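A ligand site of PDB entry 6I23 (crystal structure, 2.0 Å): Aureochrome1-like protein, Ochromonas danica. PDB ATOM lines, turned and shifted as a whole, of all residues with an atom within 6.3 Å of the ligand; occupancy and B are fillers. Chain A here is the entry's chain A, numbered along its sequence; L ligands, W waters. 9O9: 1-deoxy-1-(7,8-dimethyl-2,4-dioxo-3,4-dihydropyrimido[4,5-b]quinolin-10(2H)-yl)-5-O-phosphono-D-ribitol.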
ATOM      1  N   VAL A  19      12.253  13.008 -20.866  1.00  0.00           N
ATOM      2  CA  VAL A  19      10.959  12.506 -21.294  1.00  0.00           C
ATOM      3  C   VAL A  19       9.975  13.679 -21.417  1.00  0.00           C
ATOM      4  O   VAL A  19      10.175  14.741 -20.800  1.00  0.00           O
ATOM      5  CB  VAL A  19      10.408  11.435 -20.339  1.00  0.00           C
ATOM      6  CG1 VAL A  19      11.355  10.250 -20.275  1.00  0.00           C
ATOM      7  CG2 VAL A  19      10.169  11.943 -18.924  1.00  0.00           C
ATOM      8  N   ILE A  20       8.968  13.487 -22.272  1.00  0.00           N
ATOM      9  CA  ILE A  20       7.787  14.339 -22.374  1.00  0.00           C
ATOM     10  C   ILE A  20       6.554  13.551 -21.921  1.00  0.00           C
ATOM     11  O   ILE A  20       6.336  12.439 -22.366  1.00  0.00           O
ATOM     12  CB  ILE A  20       7.519  14.802 -23.835  1.00  0.00           C
ATOM     13  CG1 ILE A  20       8.758  15.331 -24.544  1.00  0.00           C
ATOM     14  CG2 ILE A  20       6.411  15.833 -23.898  1.00  0.00           C
ATOM     15  CD1 ILE A  20       9.221  16.651 -24.024  1.00  0.00           C
ATOM     16  N   SER A  21       5.733  14.145 -21.086  1.00  0.00           N
ATOM     17  CA  SER A  21       4.471  13.566 -20.651  1.00  0.00           C
ATOM     18  C   SER A  21       3.307  14.334 -21.211  1.00  0.00           C
ATOM     19  O   SER A  21       3.468  15.458 -21.658  1.00  0.00           O
ATOM     20  CB  SER A  21       4.381  13.513 -19.134  1.00  0.00           C
ATOM     21  OG  SER A  21       4.048  14.776 -18.626  1.00  0.00           O
ATOM     22  N   ASP A  27      -3.398   9.993 -15.647  1.00  0.00           N
ATOM     23  CA  ASP A  27      -2.114   9.721 -14.991  1.00  0.00           C
ATOM     24  C   ASP A  27      -0.828  10.282 -15.672  1.00  0.00           C
ATOM     25  O   ASP A  27       0.295   9.906 -15.292  1.00  0.00           O
ATOM     26  CB  ASP A  27      -1.928   8.227 -14.694  1.00  0.00           C
ATOM     27  CG  ASP A  27      -0.934   7.991 -13.510  1.00  0.00           C
ATOM     28  OD1 ASP A  27      -0.891   8.829 -12.580  1.00  0.00           O
ATOM     29  OD2 ASP A  27      -0.197   6.968 -13.538  1.00  0.00           O
ATOM     30  N   ASN A  28      -0.988  11.197 -16.648  1.00  0.00           N
ATOM     31  CA  ASN A  28       0.099  12.008 -17.150  1.00  0.00           C
ATOM     32  C   ASN A  28       1.312  11.144 -17.540  1.00  0.00           C
ATOM     33  O   ASN A  28       2.417  11.390 -17.044  1.00  0.00           O
ATOM     34  CB  ASN A  28       0.470  13.086 -16.074  1.00  0.00           C
ATOM     35  CG  ASN A  28       1.501  14.112 -16.564  1.00  0.00           C
ATOM     36  OD1 ASN A  28       1.546  14.469 -17.744  1.00  0.00           O
ATOM     37  ND2 ASN A  28       2.313  14.571 -15.646  1.00  0.00           N
ATOM     38  N   ILE A  30       4.287   9.147 -20.033  1.00  0.00           N
ATOM     39  CA  ILE A  30       5.302   9.446 -20.975  1.00  0.00           C
ATOM     40  C   ILE A  30       4.777   9.190 -22.403  1.00  0.00           C
ATOM     41  O   ILE A  30       4.225   8.134 -22.669  1.00  0.00           O
ATOM     42  CB  ILE A  30       6.497   8.531 -20.731  1.00  0.00           C
ATOM     43  CG1 ILE A  30       7.173   8.875 -19.404  1.00  0.00           C
ATOM     44  CG2 ILE A  30       7.550   8.653 -21.819  1.00  0.00           C
ATOM     45  CD1 ILE A  30       8.228   7.808 -19.070  1.00  0.00           C
ATOM     46  N   PHE A  37      17.700   8.801 -22.019  1.00  0.00           N
ATOM     47  CA  PHE A  37      16.903   8.393 -20.881  1.00  0.00           C
ATOM     48  C   PHE A  37      16.799   6.853 -20.836  1.00  0.00           C
ATOM     49  O   PHE A  37      16.836   6.263 -19.762  1.00  0.00           O
ATOM     50  CB  PHE A  37      15.491   9.021 -20.928  1.00  0.00           C
ATOM     51  CG  PHE A  37      14.523   8.442 -19.925  1.00  0.00           C
ATOM     52  CD1 PHE A  37      14.448   8.938 -18.635  1.00  0.00           C
ATOM     53  CD2 PHE A  37      13.692   7.394 -20.284  1.00  0.00           C
ATOM     54  CE1 PHE A  37      13.540   8.422 -17.736  1.00  0.00           C
ATOM     55  CE2 PHE A  37      12.782   6.841 -19.386  1.00  0.00           C
ATOM     56  CZ  PHE A  37      12.692   7.375 -18.100  1.00  0.00           C
ATOM     57  N   ASN A  52       3.625   6.317 -16.277  1.00  0.00           N
ATOM     58  CA  ASN A  52       4.010   7.477 -15.490  1.00  0.00           C
ATOM     59  C   ASN A  52       5.444   7.137 -15.051  1.00  0.00           C
ATOM     60  O   ASN A  52       5.723   6.015 -14.760  1.00  0.00           O
ATOM     61  CB  ASN A  52       3.071   7.634 -14.338  1.00  0.00           C
ATOM     62  CG  ASN A  52       3.385   8.830 -13.467  1.00  0.00           C
ATOM     63  OD1 ASN A  52       4.332   8.792 -12.687  1.00  0.00           O
ATOM     64  ND2 ASN A  52       2.585   9.885 -13.588  1.00  0.00           N
ATOM     65  N   CYS A  53       6.316   8.153 -14.995  1.00  0.00           N
ATOM     66  CA  CYS A  53       7.723   7.975 -14.629  1.00  0.00           C
ATOM     67  C   CYS A  53       7.969   7.641 -13.148  1.00  0.00           C
ATOM     68  O   CYS A  53       9.117   7.473 -12.762  1.00  0.00           O
ATOM     69  CB  CYS A  53       8.482   9.265 -14.981  1.00  0.00           C
ATOM     70  SG  CYS A  53       9.947   9.023 -15.993  1.00  0.00           S
ATOM     71  N   ARG A  54       6.924   7.526 -12.328  1.00  0.00           N
ATOM     72  CA  ARG A  54       7.086   7.053 -10.978  1.00  0.00           C
ATOM     73  C   ARG A  54       7.648   5.603 -10.857  1.00  0.00           C
ATOM     74  O   ARG A  54       8.080   5.201  -9.747  1.00  0.00           O
ATOM     75  CB  ARG A  54       5.809   7.193 -10.133  1.00  0.00           C
ATOM     76  CG  ARG A  54       4.772   6.093 -10.303  1.00  0.00           C
ATOM     77  CD  ARG A  54       3.633   6.298  -9.318  1.00  0.00           C
ATOM     78  NE  ARG A  54       2.820   7.488  -9.565  1.00  0.00           N
ATOM     79  CZ  ARG A  54       1.860   7.591 -10.510  1.00  0.00           C
ATOM     80  NH1 ARG A  54       1.590   6.603 -11.361  1.00  0.00           N
ATOM     81  NH2 ARG A  54       1.180   8.724 -10.629  1.00  0.00           N
ATOM     82  N   LEU A  56      10.403   4.629 -11.783  1.00  0.00           N
ATOM     83  CA  LEU A  56      11.791   4.774 -11.424  1.00  0.00           C
ATOM     84  C   LEU A  56      12.030   4.890  -9.919  1.00  0.00           C
ATOM     85  O   LEU A  56      13.178   4.805  -9.478  1.00  0.00           O
ATOM     86  CB  LEU A  56      12.364   5.990 -12.137  1.00  0.00           C
ATOM     87  CG  LEU A  56      12.397   5.910 -13.678  1.00  0.00           C
ATOM     88  CD1 LEU A  56      12.798   7.264 -14.251  1.00  0.00           C
ATOM     89  CD2 LEU A  56      13.351   4.792 -14.127  1.00  0.00           C
ATOM     90  N   GLN A  57      10.969   5.063  -9.142  1.00  0.00           N
ATOM     91  CA  GLN A  57      11.084   5.218  -7.698  1.00  0.00           C
ATOM     92  C   GLN A  57      11.023   3.835  -7.017  1.00  0.00           C
ATOM     93  O   GLN A  57      10.515   2.905  -7.605  1.00  0.00           O
ATOM     94  CB  GLN A  57       9.976   6.127  -7.205  1.00  0.00           C
ATOM     95  CG  GLN A  57      10.010   7.516  -7.855  1.00  0.00           C
ATOM     96  CD  GLN A  57       8.726   8.275  -7.676  1.00  0.00           C
ATOM     97  OE1 GLN A  57       7.866   7.898  -6.883  1.00  0.00           O
ATOM     98  NE2 GLN A  57       8.584   9.345  -8.433  1.00  0.00           N
ATOM     99  N   THR A  61      13.922   5.495  -2.214  1.00  0.00           N
ATOM    100  CA  THR A  61      13.528   6.817  -2.620  1.00  0.00           C
ATOM    101  C   THR A  61      12.781   7.532  -1.503  1.00  0.00           C
ATOM    102  O   THR A  61      11.946   6.945  -0.822  1.00  0.00           O
ATOM    103  CB  THR A  61      12.634   6.785  -3.897  1.00  0.00           C
ATOM    104  OG1 THR A  61      13.294   6.050  -4.933  1.00  0.00           O
ATOM    105  CG2 THR A  61      12.398   8.199  -4.408  1.00  0.00           C
ATOM    106  N   VAL A  66       9.583  13.119  -3.572  1.00  0.00           N
ATOM    107  CA  VAL A  66       8.497  12.816  -4.490  1.00  0.00           C
ATOM    108  C   VAL A  66       7.354  13.787  -4.230  1.00  0.00           C
ATOM    109  O   VAL A  66       6.759  14.273  -5.199  1.00  0.00           O
ATOM    110  CB  VAL A  66       7.993  11.348  -4.367  1.00  0.00           C
ATOM    111  CG1 VAL A  66       6.751  11.084  -5.235  1.00  0.00           C
ATOM    112  CG2 VAL A  66       9.130  10.420  -4.756  1.00  0.00           C
ATOM    113  N   GLU A  67       7.091  14.064  -2.947  1.00  0.00           N
ATOM    114  CA  GLU A  67       6.028  15.015  -2.514  1.00  0.00           C
ATOM    115  C   GLU A  67       6.256  16.412  -3.086  1.00  0.00           C
ATOM    116  O   GLU A  67       5.322  17.103  -3.462  1.00  0.00           O
ATOM    117  CB  GLU A  67       5.971  15.056  -0.966  1.00  0.00           C
ATOM    118  CG  GLU A  67       5.060  16.095  -0.316  1.00  0.00           C
ATOM    119  CD  GLU A  67       5.391  16.391   1.165  1.00  0.00           C
ATOM    120  OE1 GLU A  67       4.888  17.410   1.720  1.00  0.00           O
ATOM    121  OE2 GLU A  67       6.140  15.612   1.818  1.00  0.00           O
ATOM    122  N   VAL A  69       7.965  17.102  -5.913  1.00  0.00           N
ATOM    123  CA  VAL A  69       7.609  17.028  -7.340  1.00  0.00           C
ATOM    124  C   VAL A  69       6.103  17.141  -7.531  1.00  0.00           C
ATOM    125  O   VAL A  69       5.636  17.842  -8.415  1.00  0.00           O
ATOM    126  CB  VAL A  69       8.144  15.755  -7.998  1.00  0.00           C
ATOM    127  CG1 VAL A  69       7.637  15.618  -9.440  1.00  0.00           C
ATOM    128  CG2 VAL A  69       9.661  15.710  -7.970  1.00  0.00           C
ATOM    129  N   ARG A  70       5.336  16.454  -6.677  1.00  0.00           N
ATOM    130  CA  ARG A  70       3.884  16.386  -6.844  1.00  0.00           C
ATOM    131  C   ARG A  70       3.262  17.772  -6.719  1.00  0.00           C
ATOM    132  O   ARG A  70       2.433  18.163  -7.532  1.00  0.00           O
ATOM    133  CB  ARG A  70       3.253  15.417  -5.840  1.00  0.00           C
ATOM    134  CG  ARG A  70       1.765  15.171  -6.071  1.00  0.00           C
ATOM    135  CD  ARG A  70       1.070  14.351  -4.980  1.00  0.00           C
ATOM    136  NE  ARG A  70       1.674  14.468  -3.647  1.00  0.00           N
ATOM    137  CZ  ARG A  70       1.249  15.274  -2.652  1.00  0.00           C
ATOM    138  NH1 ARG A  70       1.909  15.261  -1.472  1.00  0.00           N
ATOM    139  NH2 ARG A  70       0.195  16.090  -2.804  1.00  0.00           N
ATOM    140  N   LEU A  73       4.000  20.205  -9.484  1.00  0.00           N
ATOM    141  CA  LEU A  73       3.125  19.981 -10.644  1.00  0.00           C
ATOM    142  C   LEU A  73       1.739  20.589 -10.400  1.00  0.00           C
ATOM    143  O   LEU A  73       1.212  21.251 -11.273  1.00  0.00           O
ATOM    144  CB  LEU A  73       2.992  18.495 -10.975  1.00  0.00           C
ATOM    145  CG  LEU A  73       4.256  17.795 -11.458  1.00  0.00           C
ATOM    146  CD1 LEU A  73       4.096  16.290 -11.401  1.00  0.00           C
ATOM    147  CD2 LEU A  73       4.592  18.224 -12.865  1.00  0.00           C
ATOM    148  N   LEU A  83      16.683  12.960  -6.260  1.00  0.00           N
ATOM    149  CA  LEU A  83      16.069  11.764  -5.645  1.00  0.00           C
ATOM    150  C   LEU A  83      16.723  10.461  -6.144  1.00  0.00           C
ATOM    151  O   LEU A  83      17.318  10.425  -7.250  1.00  0.00           O
ATOM    152  CB  LEU A  83      14.544  11.732  -5.805  1.00  0.00           C
ATOM    153  CG  LEU A  83      13.980  11.187  -7.147  1.00  0.00           C
ATOM    154  CD1 LEU A  83      12.471  11.224  -7.099  1.00  0.00           C
ATOM    155  CD2 LEU A  83      14.454  11.969  -8.331  1.00  0.00           C
ATOM    156  N   LEU A  84      16.633   9.430  -5.308  1.00  0.00           N
ATOM    157  CA  LEU A  84      17.108   8.092  -5.696  1.00  0.00           C
ATOM    158  C   LEU A  84      16.159   7.424  -6.709  1.00  0.00           C
ATOM    159  O   LEU A  84      14.948   7.309  -6.462  1.00  0.00           O
ATOM    160  CB  LEU A  84      17.264   7.221  -4.477  1.00  0.00           C
ATOM    161  CG  LEU A  84      18.129   5.971  -4.740  1.00  0.00           C
ATOM    162  CD1 LEU A  84      19.617   6.303  -4.815  1.00  0.00           C
ATOM    163  CD2 LEU A  84      17.850   4.911  -3.682  1.00  0.00           C
ATOM    164  N   ASN A  85      16.700   7.006  -7.843  1.00  0.00           N
ATOM    165  CA  ASN A  85      15.927   6.238  -8.798  1.00  0.00           C
ATOM    166  C   ASN A  85      16.542   4.836  -9.005  1.00  0.00           C
ATOM    167  O   ASN A  85      17.697   4.589  -8.604  1.00  0.00           O
ATOM    168  CB  ASN A  85      15.801   6.973 -10.127  1.00  0.00           C
ATOM    169  CG  ASN A  85      14.675   8.028 -10.146  1.00  0.00           C
ATOM    170  OD1 ASN A  85      14.537   8.719 -11.163  1.00  0.00           O
ATOM    171  ND2 ASN A  85      13.857   8.145  -9.063  1.00  0.00           N
ATOM    172  N   ASN A  95      19.341  11.019  -9.151  1.00  0.00           N
ATOM    173  CA  ASN A  95      18.817  11.720 -10.309  1.00  0.00           C
ATOM    174  C   ASN A  95      18.534  13.184  -9.925  1.00  0.00           C
ATOM    175  O   ASN A  95      17.693  13.442  -9.077  1.00  0.00           O
ATOM    176  CB  ASN A  95      17.562  10.957 -10.765  1.00  0.00           C
ATOM    177  CG  ASN A  95      16.845  11.602 -11.936  1.00  0.00           C
ATOM    178  OD1 ASN A  95      17.238  12.676 -12.403  1.00  0.00           O
ATOM    179  ND2 ASN A  95      15.764  10.941 -12.406  1.00  0.00           N
ATOM    180  N   LEU A  97      16.685  15.945 -11.120  1.00  0.00           N
ATOM    181  CA  LEU A  97      15.518  15.948 -11.985  1.00  0.00           C
ATOM    182  C   LEU A  97      14.954  17.372 -12.143  1.00  0.00           C
ATOM    183  O   LEU A  97      14.695  18.048 -11.168  1.00  0.00           O
ATOM    184  CB  LEU A  97      14.474  15.032 -11.363  1.00  0.00           C
ATOM    185  CG  LEU A  97      13.121  14.923 -12.052  1.00  0.00           C
ATOM    186  CD1 LEU A  97      13.301  14.424 -13.469  1.00  0.00           C
ATOM    187  CD2 LEU A  97      12.248  13.976 -11.225  1.00  0.00           C
ATOM    188  N   PHE A  98      14.781  17.814 -13.382  1.00  0.00           N
ATOM    189  CA  PHE A  98      14.292  19.120 -13.715  1.00  0.00           C
ATOM    190  C   PHE A  98      12.970  18.960 -14.458  1.00  0.00           C
ATOM    191  O   PHE A  98      12.948  18.352 -15.529  1.00  0.00           O
ATOM    192  CB  PHE A  98      15.284  19.883 -14.619  1.00  0.00           C
ATOM    193  CG  PHE A  98      16.670  20.110 -13.993  1.00  0.00           C
ATOM    194  CD1 PHE A  98      16.940  21.289 -13.200  1.00  0.00           C
ATOM    195  CD2 PHE A  98      17.736  19.196 -14.228  1.00  0.00           C
ATOM    196  CE1 PHE A  98      18.212  21.465 -12.651  1.00  0.00           C
ATOM    197  CE2 PHE A  98      19.018  19.438 -13.677  1.00  0.00           C
ATOM    198  CZ  PHE A  98      19.255  20.548 -12.909  1.00  0.00           C
ATOM    199  N   ILE A  99      11.888  19.516 -13.910  1.00  0.00           N
ATOM    200  CA  ILE A  99      10.576  19.374 -14.540  1.00  0.00           C
ATOM    201  C   ILE A  99       9.914  20.735 -14.788  1.00  0.00           C
ATOM    202  O   ILE A  99       9.833  21.552 -13.916  1.00  0.00           O
ATOM    203  CB  ILE A  99       9.656  18.480 -13.686  1.00  0.00           C
ATOM    204  CG1 ILE A  99      10.199  17.053 -13.596  1.00  0.00           C
ATOM    205  CG2 ILE A  99       8.273  18.422 -14.321  1.00  0.00           C
ATOM    206  CD1 ILE A  99       9.525  16.212 -12.563  1.00  0.00           C
ATOM    207  N   ALA A 100       9.455  20.940 -16.015  1.00  0.00           N
ATOM    208  CA  ALA A 100       8.756  22.121 -16.379  1.00  0.00           C
ATOM    209  C   ALA A 100       7.527  21.820 -17.244  1.00  0.00           C
ATOM    210  O   ALA A 100       7.537  20.943 -18.075  1.00  0.00           O
ATOM    211  CB  ALA A 100       9.693  23.039 -17.147  1.00  0.00           C
ATOM    212  N   TYR A 112       4.356  18.178 -20.106  1.00  0.00           N
ATOM    213  CA  TYR A 112       5.481  18.388 -19.180  1.00  0.00           C
ATOM    214  C   TYR A 112       6.770  17.789 -19.785  1.00  0.00           C
ATOM    215  O   TYR A 112       6.745  16.807 -20.566  1.00  0.00           O
ATOM    216  CB  TYR A 112       5.263  17.773 -17.783  1.00  0.00           C
ATOM    217  CG  TYR A 112       4.130  18.390 -17.011  1.00  0.00           C
ATOM    218  CD1 TYR A 112       4.352  19.502 -16.172  1.00  0.00           C
ATOM    219  CD2 TYR A 112       2.847  17.870 -17.077  1.00  0.00           C
ATOM    220  CE1 TYR A 112       3.307  20.105 -15.474  1.00  0.00           C
ATOM    221  CE2 TYR A 112       1.793  18.456 -16.393  1.00  0.00           C
ATOM    222  CZ  TYR A 112       2.023  19.573 -15.580  1.00  0.00           C
ATOM    223  OH  TYR A 112       0.983  20.120 -14.892  1.00  0.00           O
ATOM    224  N   LEU A 113       7.882  18.411 -19.427  1.00  0.00           N
ATOM    225  CA  LEU A 113       9.215  18.008 -19.834  1.00  0.00           C
ATOM    226  C   LEU A 113       9.993  17.713 -18.586  1.00  0.00           C
ATOM    227  O   LEU A 113      10.007  18.533 -17.684  1.00  0.00           O
ATOM    228  CB  LEU A 113       9.862  19.117 -20.615  1.00  0.00           C
ATOM    229  CG  LEU A 113      11.372  18.963 -20.975  1.00  0.00           C
ATOM    230  CD1 LEU A 113      11.652  17.858 -21.973  1.00  0.00           C
ATOM    231  CD2 LEU A 113      11.926  20.309 -21.494  1.00  0.00           C
ATOM    232  N   GLY A 114      10.610  16.551 -18.545  1.00  0.00           N
ATOM    233  CA  GLY A 114      11.531  16.183 -17.487  1.00  0.00           C
ATOM    234  C   GLY A 114      12.905  15.808 -18.026  1.00  0.00           C
ATOM    235  O   GLY A 114      12.986  15.026 -18.951  1.00  0.00           O
ATOM    236  N   VAL A 115      13.949  16.360 -17.417  1.00  0.00           N
ATOM    237  CA  VAL A 115      15.343  16.176 -17.857  1.00  0.00           C
ATOM    238  C   VAL A 115      16.039  15.577 -16.645  1.00  0.00           C
ATOM    239  O   VAL A 115      15.911  16.099 -15.518  1.00  0.00           O
ATOM    240  CB  VAL A 115      16.044  17.523 -18.201  1.00  0.00           C
ATOM    241  CG1 VAL A 115      17.521  17.310 -18.523  1.00  0.00           C
ATOM    242  CG2 VAL A 115      15.370  18.209 -19.387  1.00  0.00           C
ATOM    243  N   GLN A 116      16.702  14.445 -16.871  1.00  0.00           N
ATOM    244  CA  GLN A 116      17.441  13.743 -15.827  1.00  0.00           C
ATOM    245  C   GLN A 116      18.954  13.900 -16.022  1.00  0.00           C
ATOM    246  O   GLN A 116      19.474  13.719 -17.151  1.00  0.00           O
ATOM    247  CB  GLN A 116      17.109  12.244 -15.837  1.00  0.00           C
ATOM    248  CG  GLN A 116      15.634  11.956 -15.635  1.00  0.00           C
ATOM    249  CD  GLN A 116      14.808  12.017 -16.917  1.00  0.00           C
ATOM    250  OE1 GLN A 116      15.325  12.133 -18.030  1.00  0.00           O
ATOM    251  NE2 GLN A 116      13.504  11.913 -16.758  1.00  0.00           N
HETATM  252  C4  9O9 L   1      12.103  10.812 -13.136  1.00  0.00           C
HETATM  253  C5  9O9 L   1      10.851  11.546 -13.412  1.00  0.00           C
HETATM  254  C6  9O9 L   1       9.844  11.527 -12.334  1.00  0.00           C
HETATM  255  N1  9O9 L   1      10.117  10.852 -11.196  1.00  0.00           N
HETATM  256  N3  9O9 L   1      12.238  10.179 -11.956  1.00  0.00           N
HETATM  257  C2  9O9 L   1      11.271  10.198 -11.023  1.00  0.00           C
HETATM  258  CAA 9O9 L   1       7.962  14.300 -16.197  1.00  0.00           C
HETATM  259  CAB 9O9 L   1       6.939  14.306 -15.119  1.00  0.00           C
HETATM  260  CAC 9O9 L   1       7.172  13.630 -13.933  1.00  0.00           C
HETATM  261  CAD 9O9 L   1       8.359  12.925 -13.716  1.00  0.00           C
HETATM  262  CAE 9O9 L   1       9.384  12.908 -14.781  1.00  0.00           C
HETATM  263  CAF 9O9 L   1       9.152  13.598 -15.971  1.00  0.00           C
HETATM  264  CAJ 9O9 L   1      10.588  12.227 -14.599  1.00  0.00           C
HETATM  265  CAO 9O9 L   1       7.744  15.035 -17.502  1.00  0.00           C
HETATM  266  CAP 9O9 L   1       5.635  15.041 -15.299  1.00  0.00           C
HETATM  267  CAS 9O9 L   1       7.693  12.216 -11.391  1.00  0.00           C
HETATM  268  CAT 9O9 L   1       6.541  11.256 -11.508  1.00  0.00           C
HETATM  269  CAU 9O9 L   1       5.410  11.790 -10.639  1.00  0.00           C
HETATM  270  CAV 9O9 L   1       5.806  11.889  -9.157  1.00  0.00           C
HETATM  271  CAW 9O9 L   1       4.758  12.574  -8.291  1.00  0.00           C
HETATM  272  NAG 9O9 L   1       8.621  12.220 -12.512  1.00  0.00           N
HETATM  273  O2  9O9 L   1      11.418   9.621  -9.950  1.00  0.00           O
HETATM  274  O4  9O9 L   1      13.016  10.769 -13.977  1.00  0.00           O
HETATM  275  OAX 9O9 L   1       3.445  12.107  -8.567  1.00  0.00           O
HETATM  276  OAY 9O9 L   1       6.129  11.002 -12.869  1.00  0.00           O
HETATM  277  OAZ 9O9 L   1       6.053  10.578  -8.621  1.00  0.00           O
HETATM  278  OBA 9O9 L   1       4.923  13.063 -11.107  1.00  0.00           O
HETATM  279  OBC 9O9 L   1       2.583  11.461  -6.260  1.00  0.00           O
HETATM  280  OBD 9O9 L   1       3.597   9.714  -7.630  1.00  0.00           O
HETATM  281  OBE 9O9 L   1       1.426  10.756  -8.358  1.00  0.00           O
HETATM  282  PBB 9O9 L   1       2.737  10.969  -7.667  1.00  0.00           P
HETATM  283  O   HOH W   1       5.062  10.885 -15.685  1.00  0.00           O
HETATM  284  O   HOH W   2       5.326   7.507  -6.054  1.00  0.00           O
HETATM  285  O   HOH W   3       1.673  13.843  -9.825  1.00  0.00           O
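The backbone carbonyl oxygen (O) of Leu 83 sits at hydrogen-bond distance from the backbone NH (N) of Asn 95 (2.8 Å). OD1 of Asn 85 sits at hydrogen-bond distance from ND2 of Asn 95, at 2.8 Å. The guanidinium group (NH1) of Arg 54 lies within salt-bridge range of the side-chain carboxylate (OD2) of Asp 27. ND2 of Asn 85 sits close to O of Leu 56, 3.4 Å away. OD1 of Asn 52 sits at hydrogen-bond distance from N of Arg 54 (2.9 Å). N of Leu 113 sits at hydrogen-bond distance from O of Ala 100, at 2.9 Å. The backbone carbonyl oxygen of Tyr 112 is in hydrogen-bond range of the backbone NH of Ser 21. OD1 of Asn 28 is in hydrogen-bond range of OG of Ser 21, 2.7 Å away.
NE of Arg 54 lies within salt-bridge range of OBD of the ligand, 3.1 Å away. NE2 of Gln 116 is in hydrogen-bond range of O4 of the ligand. OD1 of Asn 85 lies within hydrogen-bond range of N3 of the ligand (2.8 Å). OAZ of the ligand lies within hydrogen-bond range of NE2 of Gln 57, 2.8 Å away. The side-chain amide nitrogen (ND2) of Asn 95 sits at hydrogen-bond distance from an oxygen (O4) of the ligand, at 3.2 Å. OD1 of Asn 52 is in hydrogen-bond range of OAY of the ligand (2.9 Å).
CG2 of Val 19 touches CAF of the ligand, at 3.5 Å. OG of Ser 21 touches CAP of the ligand (3.7 Å). Asn 28 touches the ligand (ND2 to CAP, 3.4 Å). Cys 53 touches the ligand. CD1 of Leu 56 touches O4 of the ligand, 3.5 Å away. Val 66 touches the ligand (CG1 to OAZ, 3.5 Å). CG1 of Val 69 touches CAS of the ligand, 3.9 Å away. CD of Arg 70 touches OBC of the ligand, at 3.5 Å. Leu 73 touches the ligand. CD1 of Leu 83 touches O2 of the ligand (3.4 Å). Leu 97 touches the ligand (CD2 to C5, 3.6 Å). Ile 99 touches the ligand (CD1 to CAD, 3.7 Å). Tyr 112 touches the ligand (O to CAO, 3.7 Å). Leu 113 touches the ligand (C to CAO, 3.7 Å). N of Gly 114 touches CAO of the ligand (3.4 Å). Hydrophobic or aromatic side chains within 4 Å of the ligand: Val 19, Leu 56, Val 66, Val 69, Leu 73, Leu 83, Leu 97, Ile 99 and Tyr 112. The nearest printed residue that does not touch the ligand is Phe 37 (4.5 Å).
Water W1 lies within hydrogen-bond range of OAY of the ligand (3.0 Å), O of Asn 28 (3.0 Å), N of Cys 53 (3.1 Å) and ND2 of Asn 52 (3.4 Å). Water W2 bridges OE1 of Gln 57 (2.7 Å) and OBD of the ligand (3.2 Å).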
